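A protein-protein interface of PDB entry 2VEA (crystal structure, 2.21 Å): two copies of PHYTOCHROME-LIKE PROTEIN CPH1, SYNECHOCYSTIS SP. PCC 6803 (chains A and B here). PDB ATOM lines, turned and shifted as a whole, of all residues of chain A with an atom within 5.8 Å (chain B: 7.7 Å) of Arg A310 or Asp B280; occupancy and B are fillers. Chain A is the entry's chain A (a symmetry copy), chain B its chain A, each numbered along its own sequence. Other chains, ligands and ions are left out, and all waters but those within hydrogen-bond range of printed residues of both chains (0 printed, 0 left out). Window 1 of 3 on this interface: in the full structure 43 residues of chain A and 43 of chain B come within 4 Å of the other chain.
NH1 of Arg A310 is in salt-bridge range of OD2 of Asp B280 (3.6 Å).
The side-chain carboxylate (OD2) of Asp B321 is in hydrogen-bond range of the side-chain hydroxyl (OG) of Ser A314 (2.6 Å).
The side-chain amino group (NZ) of Lys B279 sits at hydrogen-bond distance from the backbone carbonyl oxygen (O) of Ser B317, at 2.9 Å.
NZ of Lys B279 lies within salt-bridge range of OD1 of Asp B321, at 2.6 Å.
O of Val A311 sits at hydrogen-bond distance from ND2 of Asn A315.
CD2 of Phe B325 touches CD2 of Phe A307 (3.5 Å).
Phe A308 touches Phe B325.
Asp B321 touches Val A311.
CG2 of Val A311 touches CD2 of Phe B325, at 3.4 Å.
Ser A314 touches Ser B317 (OG to O, 3.9 Å).
Printed residues of chain B within 4 Å of Arg A310: Asp B280.
Of the printed residues of chain A, Asp B280 touches Arg A310.
No residue of chain B comes within 4 Å of Gly A309.
Of the printed residues of chain B, Phe A307 touches Phe B325 (3.5 Å).
Of the printed residues of chain A, Ser B317 touches Ser A314.
Asn A315 touches none of the printed residues of chain B.
Lys B279 touches none of the printed residues of chain A.
The nearest printed residue of chain B that does not touch Arg A310 is Asp B321 (5.4 Å).
The nearest printed residue of chain A that does not touch Asp B280 is Ser A314 (6.4 Å).
Of the 13 printed residues of chain A, 5 touch a printed residue of chain B.
Hydrophobic or aromatic side chains of chain A that line the printed part of chain B: Phe A307, Phe A308 and Val A311.
Among the printed residues, 7 pairs touch across the chains.
Among the printed residues, Asp or Glu carboxylates within 4 Å of a Lys or Arg side-chain nitrogen of the other chain: Arg A310 with Asp B280 (3.6 Å).
Positions printed for both chains: 277 and 313.
Of the 7 pairs that touch across the chains among the printed residues, none has its exchanged pair printed and touching as well.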
ATOM      1  N   LEU A 277      -0.287 -36.454 -20.549  1.00  0.00           N
ATOM      2  CA  LEU A 277      -0.968 -35.453 -19.726  1.00  0.00           C
ATOM      3  C   LEU A 277      -1.605 -36.073 -18.479  1.00  0.00           C
ATOM      4  O   LEU A 277      -2.443 -36.967 -18.571  1.00  0.00           O
ATOM      5  CB  LEU A 277      -2.026 -34.746 -20.556  1.00  0.00           C
ATOM      6  CG  LEU A 277      -1.466 -34.206 -21.874  1.00  0.00           C
ATOM      7  CD1 LEU A 277      -2.537 -33.469 -22.699  1.00  0.00           C
ATOM      8  CD2 LEU A 277      -0.264 -33.315 -21.583  1.00  0.00           C
ATOM      9  N   ILE A 287      -0.413 -35.974 -25.955  1.00  0.00           N
ATOM     10  CA  ILE A 287      -0.184 -35.209 -27.168  1.00  0.00           C
ATOM     11  C   ILE A 287       0.590 -36.166 -28.062  1.00  0.00           C
ATOM     12  O   ILE A 287       1.721 -36.507 -27.750  1.00  0.00           O
ATOM     13  CB  ILE A 287       0.615 -33.896 -26.933  1.00  0.00           C
ATOM     14  CG1 ILE A 287      -0.060 -33.020 -25.873  1.00  0.00           C
ATOM     15  CG2 ILE A 287       0.731 -33.101 -28.237  1.00  0.00           C
ATOM     16  CD1 ILE A 287       0.792 -31.867 -25.406  1.00  0.00           C
ATOM     17  N   CYS A 305       7.718 -28.506 -25.864  1.00  0.00           N
ATOM     18  CA  CYS A 305       6.374 -28.979 -26.235  1.00  0.00           C
ATOM     19  C   CYS A 305       5.595 -29.464 -25.036  1.00  0.00           C
ATOM     20  O   CYS A 305       4.373 -29.305 -24.972  1.00  0.00           O
ATOM     21  CB  CYS A 305       6.451 -30.124 -27.240  1.00  0.00           C
ATOM     22  SG  CYS A 305       7.125 -29.663 -28.809  1.00  0.00           S
ATOM     23  N   GLU A 306       6.302 -30.083 -24.102  1.00  0.00           N
ATOM     24  CA  GLU A 306       5.691 -30.521 -22.863  1.00  0.00           C
ATOM     25  C   GLU A 306       5.279 -29.348 -21.989  1.00  0.00           C
ATOM     26  O   GLU A 306       4.135 -29.278 -21.560  1.00  0.00           O
ATOM     27  CB  GLU A 306       6.632 -31.420 -22.067  1.00  0.00           C
ATOM     28  CG  GLU A 306       5.996 -31.894 -20.789  1.00  0.00           C
ATOM     29  CD  GLU A 306       6.962 -32.581 -19.876  1.00  0.00           C
ATOM     30  OE1 GLU A 306       8.188 -32.405 -20.050  1.00  0.00           O
ATOM     31  OE2 GLU A 306       6.484 -33.299 -18.970  1.00  0.00           O
ATOM     32  N   PHE A 307       6.204 -28.436 -21.716  1.00  0.00           N
ATOM     33  CA  PHE A 307       5.897 -27.317 -20.832  1.00  0.00           C
ATOM     34  C   PHE A 307       4.657 -26.555 -21.318  1.00  0.00           C
ATOM     35  O   PHE A 307       3.800 -26.190 -20.513  1.00  0.00           O
ATOM     36  CB  PHE A 307       7.094 -26.372 -20.683  1.00  0.00           C
ATOM     37  CG  PHE A 307       7.013 -25.486 -19.465  1.00  0.00           C
ATOM     38  CD1 PHE A 307       7.396 -25.971 -18.213  1.00  0.00           C
ATOM     39  CD2 PHE A 307       6.547 -24.175 -19.562  1.00  0.00           C
ATOM     40  CE1 PHE A 307       7.321 -25.155 -17.075  1.00  0.00           C
ATOM     41  CE2 PHE A 307       6.461 -23.352 -18.427  1.00  0.00           C
ATOM     42  CZ  PHE A 307       6.851 -23.838 -17.188  1.00  0.00           C
ATOM     43  N   PHE A 308       4.548 -26.346 -22.627  1.00  0.00           N
ATOM     44  CA  PHE A 308       3.367 -25.705 -23.190  1.00  0.00           C
ATOM     45  C   PHE A 308       2.147 -26.596 -23.032  1.00  0.00           C
ATOM     46  O   PHE A 308       1.145 -26.189 -22.432  1.00  0.00           O
ATOM     47  CB  PHE A 308       3.573 -25.375 -24.668  1.00  0.00           C
ATOM     48  CG  PHE A 308       2.393 -24.718 -25.309  1.00  0.00           C
ATOM     49  CD1 PHE A 308       2.060 -23.409 -24.995  1.00  0.00           C
ATOM     50  CD2 PHE A 308       1.617 -25.400 -26.237  1.00  0.00           C
ATOM     51  CE1 PHE A 308       0.970 -22.779 -25.597  1.00  0.00           C
ATOM     52  CE2 PHE A 308       0.524 -24.774 -26.850  1.00  0.00           C
ATOM     53  CZ  PHE A 308       0.203 -23.466 -26.521  1.00  0.00           C
ATOM     54  N   GLY A 309       2.234 -27.809 -23.573  1.00  0.00           N
ATOM     55  CA  GLY A 309       1.161 -28.786 -23.435  1.00  0.00           C
ATOM     56  C   GLY A 309       0.608 -28.841 -22.019  1.00  0.00           C
ATOM     57  O   GLY A 309      -0.605 -28.806 -21.819  1.00  0.00           O
ATOM     58  N   ARG A 310       1.512 -28.885 -21.043  1.00  0.00           N
ATOM     59  CA  ARG A 310       1.143 -28.954 -19.632  1.00  0.00           C
ATOM     60  C   ARG A 310       0.414 -27.692 -19.154  1.00  0.00           C
ATOM     61  O   ARG A 310      -0.528 -27.778 -18.380  1.00  0.00           O
ATOM     62  CB  ARG A 310       2.395 -29.198 -18.775  1.00  0.00           C
ATOM     63  CG  ARG A 310       2.132 -29.891 -17.444  1.00  0.00           C
ATOM     64  CD  ARG A 310       3.421 -30.443 -16.823  1.00  0.00           C
ATOM     65  NE  ARG A 310       3.954 -29.571 -15.776  1.00  0.00           N
ATOM     66  CZ  ARG A 310       3.541 -29.563 -14.507  1.00  0.00           C
ATOM     67  NH1 ARG A 310       4.101 -28.728 -13.639  1.00  0.00           N
ATOM     68  NH2 ARG A 310       2.571 -30.375 -14.093  1.00  0.00           N
ATOM     69  N   VAL A 311       0.843 -26.515 -19.608  1.00  0.00           N
ATOM     70  CA  VAL A 311       0.187 -25.268 -19.156  1.00  0.00           C
ATOM     71  C   VAL A 311      -1.253 -25.188 -19.635  1.00  0.00           C
ATOM     72  O   VAL A 311      -2.138 -24.736 -18.904  1.00  0.00           O
ATOM     73  CB  VAL A 311       0.897 -23.966 -19.607  1.00  0.00           C
ATOM     74  CG1 VAL A 311       0.388 -22.804 -18.788  1.00  0.00           C
ATOM     75  CG2 VAL A 311       2.387 -24.067 -19.428  1.00  0.00           C
ATOM     76  N   VAL A 312      -1.480 -25.615 -20.872  1.00  0.00           N
ATOM     77  CA  VAL A 312      -2.811 -25.565 -21.461  1.00  0.00           C
ATOM     78  C   VAL A 312      -3.633 -26.637 -20.780  1.00  0.00           C
ATOM     79  O   VAL A 312      -4.793 -26.413 -20.438  1.00  0.00           O
ATOM     80  CB  VAL A 312      -2.788 -25.806 -22.981  1.00  0.00           C
ATOM     81  CG1 VAL A 312      -4.199 -25.798 -23.535  1.00  0.00           C
ATOM     82  CG2 VAL A 312      -1.916 -24.776 -23.672  1.00  0.00           C
ATOM     83  N   PHE A 313      -3.020 -27.797 -20.551  1.00  0.00           N
ATOM     84  CA  PHE A 313      -3.708 -28.855 -19.836  1.00  0.00           C
ATOM     85  C   PHE A 313      -4.119 -28.456 -18.421  1.00  0.00           C
ATOM     86  O   PHE A 313      -5.149 -28.906 -17.928  1.00  0.00           O
ATOM     87  CB  PHE A 313      -2.907 -30.155 -19.791  1.00  0.00           C
ATOM     88  CG  PHE A 313      -3.700 -31.294 -19.257  1.00  0.00           C
ATOM     89  CD1 PHE A 313      -4.909 -31.634 -19.851  1.00  0.00           C
ATOM     90  CD2 PHE A 313      -3.274 -32.008 -18.129  1.00  0.00           C
ATOM     91  CE1 PHE A 313      -5.673 -32.661 -19.348  1.00  0.00           C
ATOM     92  CE2 PHE A 313      -4.028 -33.053 -17.625  1.00  0.00           C
ATOM     93  CZ  PHE A 313      -5.222 -33.387 -18.223  1.00  0.00           C
ATOM     94  N   SER A 314      -3.332 -27.616 -17.766  1.00  0.00           N
ATOM     95  CA  SER A 314      -3.716 -27.125 -16.449  1.00  0.00           C
ATOM     96  C   SER A 314      -5.075 -26.420 -16.567  1.00  0.00           C
ATOM     97  O   SER A 314      -5.967 -26.626 -15.736  1.00  0.00           O
ATOM     98  CB  SER A 314      -2.648 -26.182 -15.889  1.00  0.00           C
ATOM     99  OG  SER A 314      -2.900 -25.877 -14.533  1.00  0.00           O
ATOM    100  N   ASN A 315      -5.225 -25.620 -17.626  1.00  0.00           N
ATOM    101  CA  ASN A 315      -6.481 -24.937 -17.933  1.00  0.00           C
ATOM    102  C   ASN A 315      -7.593 -25.884 -18.383  1.00  0.00           C
ATOM    103  O   ASN A 315      -8.770 -25.614 -18.139  1.00  0.00           O
ATOM    104  CB  ASN A 315      -6.258 -23.858 -19.003  1.00  0.00           C
ATOM    105  CG  ASN A 315      -5.500 -22.662 -18.469  1.00  0.00           C
ATOM    106  OD1 ASN A 315      -6.052 -21.862 -17.721  1.00  0.00           O
ATOM    107  ND2 ASN A 315      -4.230 -22.533 -18.851  1.00  0.00           N
ATOM    108  N   LEU B 277      -4.931 -28.040   0.443  1.00  0.00           N
ATOM    109  CA  LEU B 277      -4.953 -27.858  -1.009  1.00  0.00           C
ATOM    110  C   LEU B 277      -3.658 -28.345  -1.667  1.00  0.00           C
ATOM    111  O   LEU B 277      -2.568 -27.876  -1.349  1.00  0.00           O
ATOM    112  CB  LEU B 277      -5.185 -26.393  -1.335  1.00  0.00           C
ATOM    113  CG  LEU B 277      -6.405 -25.821  -0.609  1.00  0.00           C
ATOM    114  CD1 LEU B 277      -6.650 -24.343  -0.962  1.00  0.00           C
ATOM    115  CD2 LEU B 277      -7.623 -26.686  -0.914  1.00  0.00           C
ATOM    116  N   ILE B 278      -3.796 -29.279  -2.599  1.00  0.00           N
ATOM    117  CA  ILE B 278      -2.639 -29.898  -3.232  1.00  0.00           C
ATOM    118  C   ILE B 278      -2.452 -29.461  -4.676  1.00  0.00           C
ATOM    119  O   ILE B 278      -3.365 -29.588  -5.491  1.00  0.00           O
ATOM    120  CB  ILE B 278      -2.755 -31.434  -3.194  1.00  0.00           C
ATOM    121  CG1 ILE B 278      -2.866 -31.919  -1.744  1.00  0.00           C
ATOM    122  CG2 ILE B 278      -1.581 -32.066  -3.895  1.00  0.00           C
ATOM    123  CD1 ILE B 278      -1.944 -31.200  -0.784  1.00  0.00           C
ATOM    124  N   LYS B 279      -1.262 -28.948  -4.977  1.00  0.00           N
ATOM    125  CA  LYS B 279      -0.838 -28.690  -6.344  1.00  0.00           C
ATOM    126  C   LYS B 279       0.286 -29.652  -6.747  1.00  0.00           C
ATOM    127  O   LYS B 279       1.326 -29.728  -6.072  1.00  0.00           O
ATOM    128  CB  LYS B 279      -0.351 -27.256  -6.476  1.00  0.00           C
ATOM    129  CG  LYS B 279       0.203 -26.941  -7.846  1.00  0.00           C
ATOM    130  CD  LYS B 279       0.073 -25.470  -8.175  1.00  0.00           C
ATOM    131  CE  LYS B 279       0.608 -25.169  -9.557  1.00  0.00           C
ATOM    132  NZ  LYS B 279      -0.192 -24.101 -10.172  1.00  0.00           N
ATOM    133  N   ASP B 280       0.077 -30.373  -7.849  1.00  0.00           N
ATOM    134  CA  ASP B 280       1.085 -31.292  -8.391  1.00  0.00           C
ATOM    135  C   ASP B 280       1.689 -32.163  -7.266  1.00  0.00           C
ATOM    136  O   ASP B 280       2.905 -32.341  -7.189  1.00  0.00           O
ATOM    137  CB  ASP B 280       2.196 -30.517  -9.139  1.00  0.00           C
ATOM    138  CG  ASP B 280       1.653 -29.408 -10.075  1.00  0.00           C
ATOM    139  OD1 ASP B 280       0.462 -29.446 -10.477  1.00  0.00           O
ATOM    140  OD2 ASP B 280       2.437 -28.485 -10.415  1.00  0.00           O
ATOM    141  N   GLY B 281       0.834 -32.667  -6.375  1.00  0.00           N
ATOM    142  CA  GLY B 281       1.261 -33.550  -5.290  1.00  0.00           C
ATOM    143  C   GLY B 281       2.094 -32.951  -4.161  1.00  0.00           C
ATOM    144  O   GLY B 281       2.775 -33.683  -3.431  1.00  0.00           O
ATOM    145  N   HIS B 282       2.057 -31.631  -4.012  1.00  0.00           N
ATOM    146  CA  HIS B 282       2.701 -30.960  -2.876  1.00  0.00           C
ATOM    147  C   HIS B 282       1.703 -30.043  -2.158  1.00  0.00           C
ATOM    148  O   HIS B 282       0.757 -29.535  -2.768  1.00  0.00           O
ATOM    149  CB  HIS B 282       3.925 -30.159  -3.336  1.00  0.00           C
ATOM    150  N   LEU B 283       1.922 -29.859  -0.857  1.00  0.00           N
ATOM    151  CA  LEU B 283       1.034 -29.056  -0.030  1.00  0.00           C
ATOM    152  C   LEU B 283       1.191 -27.580  -0.376  1.00  0.00           C
ATOM    153  O   LEU B 283       2.178 -26.941  -0.012  1.00  0.00           O
ATOM    154  CB  LEU B 283       1.317 -29.294   1.455  1.00  0.00           C
ATOM    155  CG  LEU B 283       0.291 -28.741   2.449  1.00  0.00           C
ATOM    156  CD1 LEU B 283      -1.111 -29.220   2.129  1.00  0.00           C
ATOM    157  CD2 LEU B 283       0.673 -29.142   3.858  1.00  0.00           C
ATOM    158  N   TRP B 284       0.211 -27.049  -1.097  1.00  0.00           N
ATOM    159  CA  TRP B 284       0.224 -25.655  -1.512  1.00  0.00           C
ATOM    160  C   TRP B 284      -0.205 -24.804  -0.337  1.00  0.00           C
ATOM    161  O   TRP B 284       0.473 -23.847   0.019  1.00  0.00           O
ATOM    162  CB  TRP B 284      -0.721 -25.466  -2.695  1.00  0.00           C
ATOM    163  CG  TRP B 284      -0.806 -24.090  -3.252  1.00  0.00           C
ATOM    164  CD1 TRP B 284      -0.081 -23.580  -4.287  1.00  0.00           C
ATOM    165  CD2 TRP B 284      -1.701 -23.055  -2.840  1.00  0.00           C
ATOM    166  NE1 TRP B 284      -0.457 -22.286  -4.535  1.00  0.00           N
ATOM    167  CE2 TRP B 284      -1.457 -21.940  -3.667  1.00  0.00           C
ATOM    168  CE3 TRP B 284      -2.689 -22.961  -1.856  1.00  0.00           C
ATOM    169  CZ2 TRP B 284      -2.164 -20.740  -3.538  1.00  0.00           C
ATOM    170  CZ3 TRP B 284      -3.396 -21.767  -1.728  1.00  0.00           C
ATOM    171  CH2 TRP B 284      -3.117 -20.671  -2.560  1.00  0.00           C
ATOM    172  N   PHE B 313      -9.663 -24.128  -6.243  1.00  0.00           N
ATOM    173  CA  PHE B 313      -8.227 -24.329  -6.289  1.00  0.00           C
ATOM    174  C   PHE B 313      -7.736 -24.862  -7.633  1.00  0.00           C
ATOM    175  O   PHE B 313      -6.633 -24.536  -8.059  1.00  0.00           O
ATOM    176  CB  PHE B 313      -7.721 -25.230  -5.163  1.00  0.00           C
ATOM    177  CG  PHE B 313      -6.237 -25.255  -5.077  1.00  0.00           C
ATOM    178  CD1 PHE B 313      -5.532 -24.066  -4.935  1.00  0.00           C
ATOM    179  CD2 PHE B 313      -5.526 -26.456  -5.185  1.00  0.00           C
ATOM    180  CE1 PHE B 313      -4.157 -24.067  -4.891  1.00  0.00           C
ATOM    181  CE2 PHE B 313      -4.142 -26.470  -5.126  1.00  0.00           C
ATOM    182  CZ  PHE B 313      -3.452 -25.288  -4.979  1.00  0.00           C
ATOM    183  N   SER B 317      -4.731 -23.005  -9.386  1.00  0.00           N
ATOM    184  CA  SER B 317      -3.576 -23.694  -9.930  1.00  0.00           C
ATOM    185  C   SER B 317      -3.399 -23.370 -11.403  1.00  0.00           C
ATOM    186  O   SER B 317      -2.288 -23.124 -11.854  1.00  0.00           O
ATOM    187  CB  SER B 317      -3.720 -25.203  -9.739  1.00  0.00           C
ATOM    188  OG  SER B 317      -2.705 -25.893 -10.440  1.00  0.00           O
ATOM    189  N   GLU B 320      -2.079 -19.544 -11.789  1.00  0.00           N
ATOM    190  CA  GLU B 320      -0.685 -19.347 -11.432  1.00  0.00           C
ATOM    191  C   GLU B 320       0.224 -20.109 -12.405  1.00  0.00           C
ATOM    192  O   GLU B 320       1.295 -19.625 -12.752  1.00  0.00           O
ATOM    193  CB  GLU B 320      -0.421 -19.663  -9.950  1.00  0.00           C
ATOM    194  CG  GLU B 320      -0.546 -21.100  -9.535  1.00  0.00           C
ATOM    195  CD  GLU B 320      -0.270 -21.301  -8.047  1.00  0.00           C
ATOM    196  OE1 GLU B 320      -0.646 -20.427  -7.232  1.00  0.00           O
ATOM    197  OE2 GLU B 320       0.333 -22.341  -7.701  1.00  0.00           O
ATOM    198  N   ASP B 321      -0.222 -21.267 -12.882  1.00  0.00           N
ATOM    199  CA  ASP B 321       0.494 -21.959 -13.956  1.00  0.00           C
ATOM    200  C   ASP B 321       0.632 -21.079 -15.188  1.00  0.00           C
ATOM    201  O   ASP B 321       1.711 -20.991 -15.767  1.00  0.00           O
ATOM    202  CB  ASP B 321      -0.192 -23.274 -14.342  1.00  0.00           C
ATOM    203  CG  ASP B 321       0.112 -24.401 -13.374  1.00  0.00           C
ATOM    204  OD1 ASP B 321       0.991 -24.227 -12.504  1.00  0.00           O
ATOM    205  OD2 ASP B 321      -0.528 -25.466 -13.487  1.00  0.00           O
ATOM    206  N   PHE B 325       4.010 -19.434 -16.884  1.00  0.00           N
ATOM    207  CA  PHE B 325       4.364 -19.596 -18.297  1.00  0.00           C
ATOM    208  C   PHE B 325       4.569 -18.246 -18.972  1.00  0.00           C
ATOM    209  O   PHE B 325       5.402 -18.115 -19.865  1.00  0.00           O
ATOM    210  CB  PHE B 325       3.274 -20.383 -19.032  1.00  0.00           C
ATOM    211  CG  PHE B 325       3.598 -20.681 -20.470  1.00  0.00           C
ATOM    212  CD1 PHE B 325       3.013 -19.956 -21.500  1.00  0.00           C
ATOM    213  CD2 PHE B 325       4.482 -21.693 -20.794  1.00  0.00           C
ATOM    214  CE1 PHE B 325       3.311 -20.237 -22.823  1.00  0.00           C
ATOM    215  CE2 PHE B 325       4.787 -21.985 -22.115  1.00  0.00           C
ATOM    216  CZ  PHE B 325       4.201 -21.254 -23.132  1.00  0.00           C
